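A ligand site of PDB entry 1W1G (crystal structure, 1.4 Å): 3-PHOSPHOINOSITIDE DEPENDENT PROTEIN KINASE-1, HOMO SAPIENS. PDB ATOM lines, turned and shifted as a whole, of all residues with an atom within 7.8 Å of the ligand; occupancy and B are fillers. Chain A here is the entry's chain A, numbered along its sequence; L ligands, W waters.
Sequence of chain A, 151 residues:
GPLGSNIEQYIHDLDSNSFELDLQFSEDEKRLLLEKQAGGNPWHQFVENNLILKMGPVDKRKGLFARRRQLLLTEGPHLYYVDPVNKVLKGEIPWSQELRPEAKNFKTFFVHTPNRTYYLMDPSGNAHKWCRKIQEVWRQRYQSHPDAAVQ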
ATOM      1  N   LYS A  60      19.254  31.671 -29.283  1.00  0.00           N
ATOM      2  CA  LYS A  60      20.422  30.811 -29.068  1.00  0.00           C
ATOM      3  C   LYS A  60      20.814  30.183 -30.402  1.00  0.00           C
ATOM      4  O   LYS A  60      20.038  29.443 -31.003  1.00  0.00           O
ATOM      5  CB  LYS A  60      20.146  29.694 -28.071  1.00  0.00           C
ATOM      6  CG  LYS A  60      21.267  28.703 -27.910  1.00  0.00           C
ATOM      7  CD  LYS A  60      21.165  27.900 -26.568  1.00  0.00           C
ATOM      8  CE  LYS A  60      19.818  27.211 -26.405  1.00  0.00           C
ATOM      9  NZ  LYS A  60      19.440  26.180 -27.441  1.00  0.00           N
ATOM     10  N   ARG A  61      21.993  30.547 -30.848  1.00  0.00           N
ATOM     11  CA  ARG A  61      22.530  30.100 -32.113  1.00  0.00           C
ATOM     12  C   ARG A  61      23.061  28.697 -31.984  1.00  0.00           C
ATOM     13  O   ARG A  61      23.801  28.400 -31.042  1.00  0.00           O
ATOM     14  CB  ARG A  61      23.688  30.999 -32.513  1.00  0.00           C
ATOM     15  CG  ARG A  61      23.252  32.362 -32.919  1.00  0.00           C
ATOM     16  CD  ARG A  61      22.991  32.486 -34.426  1.00  0.00           C
ATOM     17  NE  ARG A  61      24.270  32.495 -35.116  1.00  0.00           N
ATOM     18  CZ  ARG A  61      24.757  31.509 -35.844  1.00  0.00           C
ATOM     19  NH1 ARG A  61      24.054  30.394 -36.075  1.00  0.00           N
ATOM     20  NH2 ARG A  61      25.941  31.653 -36.389  1.00  0.00           N
ATOM     21  N   LYS A  62      22.721  27.839 -32.941  1.00  0.00           N
ATOM     22  CA  LYS A  62      23.261  26.472 -33.000  1.00  0.00           C
ATOM     23  C   LYS A  62      23.013  26.029 -34.454  1.00  0.00           C
ATOM     24  O   LYS A  62      21.888  26.098 -34.974  1.00  0.00           O
ATOM     25  CB  LYS A  62      22.537  25.564 -31.998  1.00  0.00           C
ATOM     26  CG  LYS A  62      23.195  24.228 -31.573  1.00  0.00           C
ATOM     27  CD  LYS A  62      24.714  24.265 -31.567  1.00  0.00           C
ATOM     28  CE  LYS A  62      25.319  23.069 -30.862  1.00  0.00           C
ATOM     29  NZ  LYS A  62      25.268  21.782 -31.636  1.00  0.00           N
ATOM     30  N   GLY A  63      24.057  25.629 -35.154  1.00  0.00           N
ATOM     31  CA  GLY A  63      23.914  25.343 -36.559  1.00  0.00           C
ATOM     32  C   GLY A  63      23.941  26.653 -37.311  1.00  0.00           C
ATOM     33  O   GLY A  63      24.587  27.593 -36.869  1.00  0.00           O
ATOM     34  N   LEU A  64      23.345  26.695 -38.494  1.00  0.00           N
ATOM     35  CA  LEU A  64      23.334  27.937 -39.268  1.00  0.00           C
ATOM     36  C   LEU A  64      22.460  28.983 -38.638  1.00  0.00           C
ATOM     37  O   LEU A  64      22.657  30.164 -38.887  1.00  0.00           O
ATOM     38  CB  LEU A  64      22.802  27.703 -40.694  1.00  0.00           C
ATOM     39  CG  LEU A  64      23.697  26.927 -41.626  1.00  0.00           C
ATOM     40  CD1 LEU A  64      22.995  26.766 -43.000  1.00  0.00           C
ATOM     41  CD2 LEU A  64      25.004  27.666 -41.756  1.00  0.00           C
ATOM     42  N   PHE A  65      21.413  28.579 -37.910  1.00  0.00           N
ATOM     43  CA  PHE A  65      20.478  29.583 -37.410  1.00  0.00           C
ATOM     44  C   PHE A  65      20.342  29.576 -35.875  1.00  0.00           C
ATOM     45  O   PHE A  65      21.358  29.469 -35.166  1.00  0.00           O
ATOM     46  CB  PHE A  65      19.178  29.455 -38.198  1.00  0.00           C
ATOM     47  CG  PHE A  65      19.407  29.506 -39.686  1.00  0.00           C
ATOM     48  CD1 PHE A  65      19.955  30.644 -40.284  1.00  0.00           C
ATOM     49  CD2 PHE A  65      19.220  28.378 -40.503  1.00  0.00           C
ATOM     50  CE1 PHE A  65      20.216  30.705 -41.645  1.00  0.00           C
ATOM     51  CE2 PHE A  65      19.481  28.421 -41.873  1.00  0.00           C
ATOM     52  CZ  PHE A  65      19.999  29.584 -42.453  1.00  0.00           C
ATOM     53  N   ALA A  66      19.114  29.683 -35.393  1.00  0.00           N
ATOM     54  CA  ALA A  66      18.885  29.845 -33.959  1.00  0.00           C
ATOM     55  C   ALA A  66      17.456  29.505 -33.581  1.00  0.00           C
ATOM     56  O   ALA A  66      16.556  29.325 -34.430  1.00  0.00           O
ATOM     57  CB  ALA A  66      19.215  31.251 -33.538  1.00  0.00           C
ATOM     58  N   ARG A  67      17.214  29.511 -32.278  1.00  0.00           N
ATOM     59  CA  ARG A  67      15.894  29.295 -31.731  1.00  0.00           C
ATOM     60  C   ARG A  67      15.693  30.340 -30.630  1.00  0.00           C
ATOM     61  O   ARG A  67      16.635  30.626 -29.888  1.00  0.00           O
ATOM     62  CB  ARG A  67      15.768  27.896 -31.128  1.00  0.00           C
ATOM     63  CG  ARG A  67      15.865  26.798 -32.198  1.00  0.00           C
ATOM     64  CD  ARG A  67      14.756  26.805 -33.203  1.00  0.00           C
ATOM     65  NE  ARG A  67      14.836  25.687 -34.155  1.00  0.00           N
ATOM     66  CZ  ARG A  67      14.125  25.589 -35.273  1.00  0.00           C
ATOM     67  NH1 ARG A  67      13.317  26.568 -35.632  1.00  0.00           N
ATOM     68  NH2 ARG A  67      14.258  24.530 -36.061  1.00  0.00           N
ATOM     69  N   ARG A  68      14.524  30.974 -30.601  1.00  0.00           N
ATOM     70  CA  ARG A  68      14.193  31.932 -29.553  1.00  0.00           C
ATOM     71  C   ARG A  68      13.821  31.142 -28.281  1.00  0.00           C
ATOM     72  O   ARG A  68      12.901  30.282 -28.295  1.00  0.00           O
ATOM     73  CB  ARG A  68      13.014  32.783 -29.978  1.00  0.00           C
ATOM     74  CG  ARG A  68      12.375  33.603 -28.872  1.00  0.00           C
ATOM     75  CD  ARG A  68      13.271  34.603 -28.305  1.00  0.00           C
ATOM     76  NE  ARG A  68      13.814  35.565 -29.264  1.00  0.00           N
ATOM     77  CZ  ARG A  68      13.281  36.751 -29.559  1.00  0.00           C
ATOM     78  NH1 ARG A  68      12.087  37.133 -29.056  1.00  0.00           N
ATOM     79  NH2 ARG A  68      13.907  37.547 -30.403  1.00  0.00           N
ATOM     80  N   ARG A  69      14.504  31.468 -27.182  1.00  0.00           N
ATOM     81  CA  ARG A  69      14.224  30.831 -25.896  1.00  0.00           C
ATOM     82  C   ARG A  69      14.073  31.883 -24.786  1.00  0.00           C
ATOM     83  O   ARG A  69      14.602  32.981 -24.898  1.00  0.00           O
ATOM     84  CB  ARG A  69      15.343  29.902 -25.517  1.00  0.00           C
ATOM     85  CG  ARG A  69      15.605  28.808 -26.549  1.00  0.00           C
ATOM     86  CD  ARG A  69      14.601  27.739 -26.437  1.00  0.00           C
ATOM     87  NE  ARG A  69      14.625  26.725 -27.474  1.00  0.00           N
ATOM     88  CZ  ARG A  69      13.720  26.591 -28.447  1.00  0.00           C
ATOM     89  NH1 ARG A  69      12.719  27.445 -28.607  1.00  0.00           N
ATOM     90  NH2 ARG A  69      13.807  25.561 -29.270  1.00  0.00           N
ATOM     91  N   TYR A  81      16.831  27.311 -20.112  1.00  0.00           N
ATOM     92  CA  TYR A  81      16.198  27.907 -21.283  1.00  0.00           C
ATOM     93  C   TYR A  81      14.941  27.124 -21.691  1.00  0.00           C
ATOM     94  O   TYR A  81      14.949  25.902 -21.735  1.00  0.00           O
ATOM     95  CB  TYR A  81      17.186  28.111 -22.435  1.00  0.00           C
ATOM     96  CG  TYR A  81      18.014  26.916 -22.819  1.00  0.00           C
ATOM     97  CD1 TYR A  81      19.296  26.693 -22.245  1.00  0.00           C
ATOM     98  CD2 TYR A  81      17.548  26.018 -23.746  1.00  0.00           C
ATOM     99  CE1 TYR A  81      20.041  25.590 -22.590  1.00  0.00           C
ATOM    100  CE2 TYR A  81      18.320  24.922 -24.125  1.00  0.00           C
ATOM    101  CZ  TYR A  81      19.543  24.699 -23.532  1.00  0.00           C
ATOM    102  OH  TYR A  81      20.265  23.618 -23.896  1.00  0.00           O
ATOM    103  N   VAL A  82      13.916  27.874 -22.055  1.00  0.00           N
ATOM    104  CA  VAL A  82      12.601  27.347 -22.268  1.00  0.00           C
ATOM    105  C   VAL A  82      12.071  27.753 -23.650  1.00  0.00           C
ATOM    106  O   VAL A  82      12.262  28.871 -24.095  1.00  0.00           O
ATOM    107  CB  VAL A  82      11.667  27.959 -21.225  1.00  0.00           C
ATOM    108  CG1 VAL A  82      10.231  27.520 -21.475  1.00  0.00           C
ATOM    109  CG2 VAL A  82      12.108  27.599 -19.804  1.00  0.00           C
ATOM    110  N   ASP A  83      11.352  26.845 -24.295  1.00  0.00           N
ATOM    111  CA  ASP A  83      10.610  27.185 -25.523  1.00  0.00           C
ATOM    112  C   ASP A  83       9.361  27.988 -25.182  1.00  0.00           C
ATOM    113  O   ASP A  83       8.467  27.453 -24.525  1.00  0.00           O
ATOM    114  CB  ASP A  83      10.275  25.873 -26.237  1.00  0.00           C
ATOM    115  CG  ASP A  83       9.434  26.059 -27.456  1.00  0.00           C
ATOM    116  OD1 ASP A  83       8.852  27.163 -27.686  1.00  0.00           O
ATOM    117  OD2 ASP A  83       9.286  25.109 -28.260  1.00  0.00           O
ATOM    118  N   VAL A  88       7.751  24.557 -22.989  1.00  0.00           N
ATOM    119  CA  VAL A  88       8.482  23.371 -22.526  1.00  0.00           C
ATOM    120  C   VAL A  88       9.958  23.729 -22.233  1.00  0.00           C
ATOM    121  O   VAL A  88      10.626  24.449 -23.021  1.00  0.00           O
ATOM    122  CB  VAL A  88       8.430  22.241 -23.603  1.00  0.00           C
ATOM    123  CG1 VAL A  88       8.330  22.828 -24.992  1.00  0.00           C
ATOM    124  CG2 VAL A  88       9.660  21.306 -23.520  1.00  0.00           C
ATOM    125  N   LEU A  89      10.469  23.209 -21.118  1.00  0.00           N
ATOM    126  CA  LEU A  89      11.883  23.341 -20.792  1.00  0.00           C
ATOM    127  C   LEU A  89      12.689  22.634 -21.870  1.00  0.00           C
ATOM    128  O   LEU A  89      12.417  21.463 -22.158  1.00  0.00           O
ATOM    129  CB  LEU A  89      12.194  22.734 -19.421  1.00  0.00           C
ATOM    130  CG  LEU A  89      13.651  22.807 -19.007  1.00  0.00           C
ATOM    131  CD1 LEU A  89      14.057  24.272 -18.794  1.00  0.00           C
ATOM    132  CD2 LEU A  89      13.945  21.997 -17.746  1.00  0.00           C
ATOM    133  N   LYS A  90      13.682  23.311 -22.451  1.00  0.00           N
ATOM    134  CA  LYS A  90      14.540  22.680 -23.460  1.00  0.00           C
ATOM    135  C   LYS A  90      15.899  22.289 -22.932  1.00  0.00           C
ATOM    136  O   LYS A  90      16.506  21.349 -23.432  1.00  0.00           O
ATOM    137  CB  LYS A  90      14.708  23.567 -24.685  1.00  0.00           C
ATOM    138  CG  LYS A  90      13.404  23.894 -25.405  1.00  0.00           C
ATOM    139  CD  LYS A  90      12.687  22.675 -25.945  1.00  0.00           C
ATOM    140  CE  LYS A  90      13.470  21.902 -26.988  1.00  0.00           C
ATOM    141  NZ  LYS A  90      12.728  20.632 -27.311  1.00  0.00           N
ATOM    142  N   GLY A  91      16.414  23.003 -21.941  1.00  0.00           N
ATOM    143  CA  GLY A  91      17.681  22.611 -21.332  1.00  0.00           C
ATOM    144  C   GLY A  91      18.161  23.617 -20.290  1.00  0.00           C
ATOM    145  O   GLY A  91      17.419  24.537 -19.943  1.00  0.00           O
ATOM    146  N   GLU A  92      19.401  23.392 -19.837  1.00  0.00           N
ATOM    147  CA  GLU A  92      20.179  24.327 -18.991  1.00  0.00           C
ATOM    148  C   GLU A  92      21.607  24.490 -19.502  1.00  0.00           C
ATOM    149  O   GLU A  92      22.181  23.576 -20.110  1.00  0.00           O
ATOM    150  CB  GLU A  92      20.318  23.826 -17.549  1.00  0.00           C
ATOM    151  CG  GLU A  92      19.052  23.555 -16.798  1.00  0.00           C
ATOM    152  CD  GLU A  92      19.378  23.103 -15.378  1.00  0.00           C
ATOM    153  OE1 GLU A  92      20.156  23.811 -14.680  1.00  0.00           O
ATOM    154  OE2 GLU A  92      18.865  22.035 -14.989  1.00  0.00           O
ATOM    155  N   ARG A 116      31.373  23.151 -24.036  1.00  0.00           N
ATOM    156  CA  ARG A 116      30.543  23.851 -25.007  1.00  0.00           C
ATOM    157  C   ARG A 116      30.465  25.330 -24.685  1.00  0.00           C
ATOM    158  O   ARG A 116      30.387  25.716 -23.506  1.00  0.00           O
ATOM    159  CB  ARG A 116      29.133  23.277 -24.991  1.00  0.00           C
ATOM    160  CG  ARG A 116      28.186  24.064 -25.852  1.00  0.00           C
ATOM    161  CD  ARG A 116      26.927  23.346 -26.132  1.00  0.00           C
ATOM    162  NE  ARG A 116      26.003  24.221 -26.821  1.00  0.00           N
ATOM    163  CZ  ARG A 116      24.707  23.961 -26.958  1.00  0.00           C
ATOM    164  NH1 ARG A 116      24.198  22.822 -26.481  1.00  0.00           N
ATOM    165  NH2 ARG A 116      23.931  24.845 -27.558  1.00  0.00           N
ATOM    166  N   TYR A 118      27.949  28.549 -25.388  1.00  0.00           N
ATOM    167  CA  TYR A 118      26.585  28.881 -25.809  1.00  0.00           C
ATOM    168  C   TYR A 118      26.607  30.275 -26.446  1.00  0.00           C
ATOM    169  O   TYR A 118      27.213  31.191 -25.920  1.00  0.00           O
ATOM    170  CB  TYR A 118      25.611  28.824 -24.613  1.00  0.00           C
ATOM    171  CG  TYR A 118      25.420  27.392 -24.077  1.00  0.00           C
ATOM    172  CD1 TYR A 118      26.397  26.768 -23.303  1.00  0.00           C
ATOM    173  CD2 TYR A 118      24.263  26.672 -24.349  1.00  0.00           C
ATOM    174  CE1 TYR A 118      26.200  25.474 -22.829  1.00  0.00           C
ATOM    175  CE2 TYR A 118      24.077  25.373 -23.868  1.00  0.00           C
ATOM    176  CZ  TYR A 118      25.061  24.786 -23.097  1.00  0.00           C
ATOM    177  OH  TYR A 118      24.894  23.494 -22.626  1.00  0.00           O
HETATM  178  O1  LIG L   1      18.847  19.307 -37.721  1.00  0.00           O
HETATM  179  C1  LIG L   1      18.139  18.350 -36.897  1.00  0.00           C
HETATM  180  C2  LIG L   1      17.171  19.118 -35.993  1.00  0.00           C
HETATM  181  O2  LIG L   1      16.604  18.239 -35.019  1.00  0.00           O
HETATM  182  C3  LIG L   1      17.876  20.249 -35.235  1.00  0.00           C
HETATM  183  O3  LIG L   1      16.902  21.006 -34.497  1.00  0.00           O
HETATM  184  P1  LIG L   1      17.044  22.573 -34.433  1.00  0.00           P
HETATM  185  O4  LIG L   1      15.781  23.059 -33.540  1.00  0.00           O
HETATM  186  O5  LIG L   1      17.096  23.208 -35.781  1.00  0.00           O
HETATM  187  O6  LIG L   1      18.406  22.873 -33.707  1.00  0.00           O
HETATM  188  C4  LIG L   1      18.524  22.429 -32.346  1.00  0.00           C
HETATM  189  C5  LIG L   1      18.206  23.561 -31.343  1.00  0.00           C
HETATM  190  O7  LIG L   1      19.100  24.666 -31.523  1.00  0.00           O
HETATM  191  C6  LIG L   1      18.439  23.025 -29.898  1.00  0.00           C
HETATM  192  O8  LIG L   1      18.201  24.075 -28.951  1.00  0.00           O
HETATM  193  P2  LIG L   1      16.985  23.773 -27.937  1.00  0.00           P
HETATM  194  O9  LIG L   1      15.667  23.579 -28.748  1.00  0.00           O
HETATM  195  O10 LIG L   1      16.886  25.146 -27.095  1.00  0.00           O
HETATM  196  O11 LIG L   1      17.234  22.527 -27.106  1.00  0.00           O
HETATM  197  C7  LIG L   1      19.874  22.532 -29.679  1.00  0.00           C
HETATM  198  O12 LIG L   1      19.996  21.886 -28.408  1.00  0.00           O
HETATM  199  P3  LIG L   1      20.621  22.733 -27.139  1.00  0.00           P
HETATM  200  O13 LIG L   1      19.386  22.655 -26.159  1.00  0.00           O
HETATM  201  O14 LIG L   1      21.824  21.834 -26.710  1.00  0.00           O
HETATM  202  O15 LIG L   1      21.181  24.080 -27.577  1.00  0.00           O
HETATM  203  C8  LIG L   1      20.252  21.461 -30.750  1.00  0.00           C
HETATM  204  O16 LIG L   1      21.653  21.307 -30.649  1.00  0.00           O
HETATM  205  P4  LIG L   1      22.244  19.982 -29.876  1.00  0.00           P
HETATM  206  O17 LIG L   1      23.114  20.643 -28.698  1.00  0.00           O
HETATM  207  O18 LIG L   1      23.342  19.357 -30.788  1.00  0.00           O
HETATM  208  O19 LIG L   1      21.125  19.138 -29.347  1.00  0.00           O
HETATM  209  C9  LIG L   1      19.936  21.940 -32.157  1.00  0.00           C
HETATM  210  O20 LIG L   1      20.172  20.838 -33.052  1.00  0.00           O
HETATM  211  O   HOH W   1      19.096  26.975 -30.016  1.00  0.00           O
HETATM  212  O   HOH W   2      15.785  19.994 -25.993  1.00  0.00           O
HETATM  213  O   HOH W   3      14.874  22.049 -30.934  1.00  0.00           O
HETATM  214  O   HOH W   4      18.088  25.631 -35.902  1.00  0.00           O
HETATM  215  O   HOH W   5      19.358  26.274 -33.674  1.00  0.00           O
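Water W5 bridges an oxygen (O7) of the ligand (2.7 Å) and the backbone carbonyl oxygen (O) of Lys 62 (2.8 Å).
Water W1 bridges the side-chain amino group of Lys 60 (2.7 Å) and an oxygen (O7) of the ligand (2.8 Å).
Water W2 bridges O of Lys 90 and O11 of the ligand.
Merely in contact with the ligand: Lys 90 (3.3 Å).
Hydrophobic or aromatic side chains that line the ligand: Tyr 81.
Of the 20 residues printed, 7 come within 4 Å of the ligand.
The backbone NH of Lys 90 sits at hydrogen-bond distance from the backbone carbonyl oxygen of Tyr 81, at 3.0 Å.
O of Gly 91 is in hydrogen-bond range of N of Tyr 81 (2.8 Å).
The guanidinium group (NH1) of Arg 69 lies within salt-bridge range of the side-chain carboxylate (OD1) of Asp 83 (3.99 Å).
The backbone carbonyl oxygen (O) of Arg 67 is in hydrogen-bond range of the backbone NH (N) of Lys 60 (2.9 Å).
An oxygen (O9) of the ligand is in salt-bridge range of the guanidinium group of Arg 69 (2.8 Å).
O18 of the ligand lies within salt-bridge range of NZ of Lys 62, at 3.2 Å.
The side-chain amino group of Lys 60 lies within salt-bridge range of an oxygen (O15) of the ligand (2.7 Å).
NH1 of Arg 116 lies within salt-bridge range of O14 of the ligand (2.6 Å).
O4 of the ligand lies within salt-bridge range of NE of Arg 67, 2.9 Å away.
OH of Tyr 81 lies within hydrogen-bond range of O13 of the ligand.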
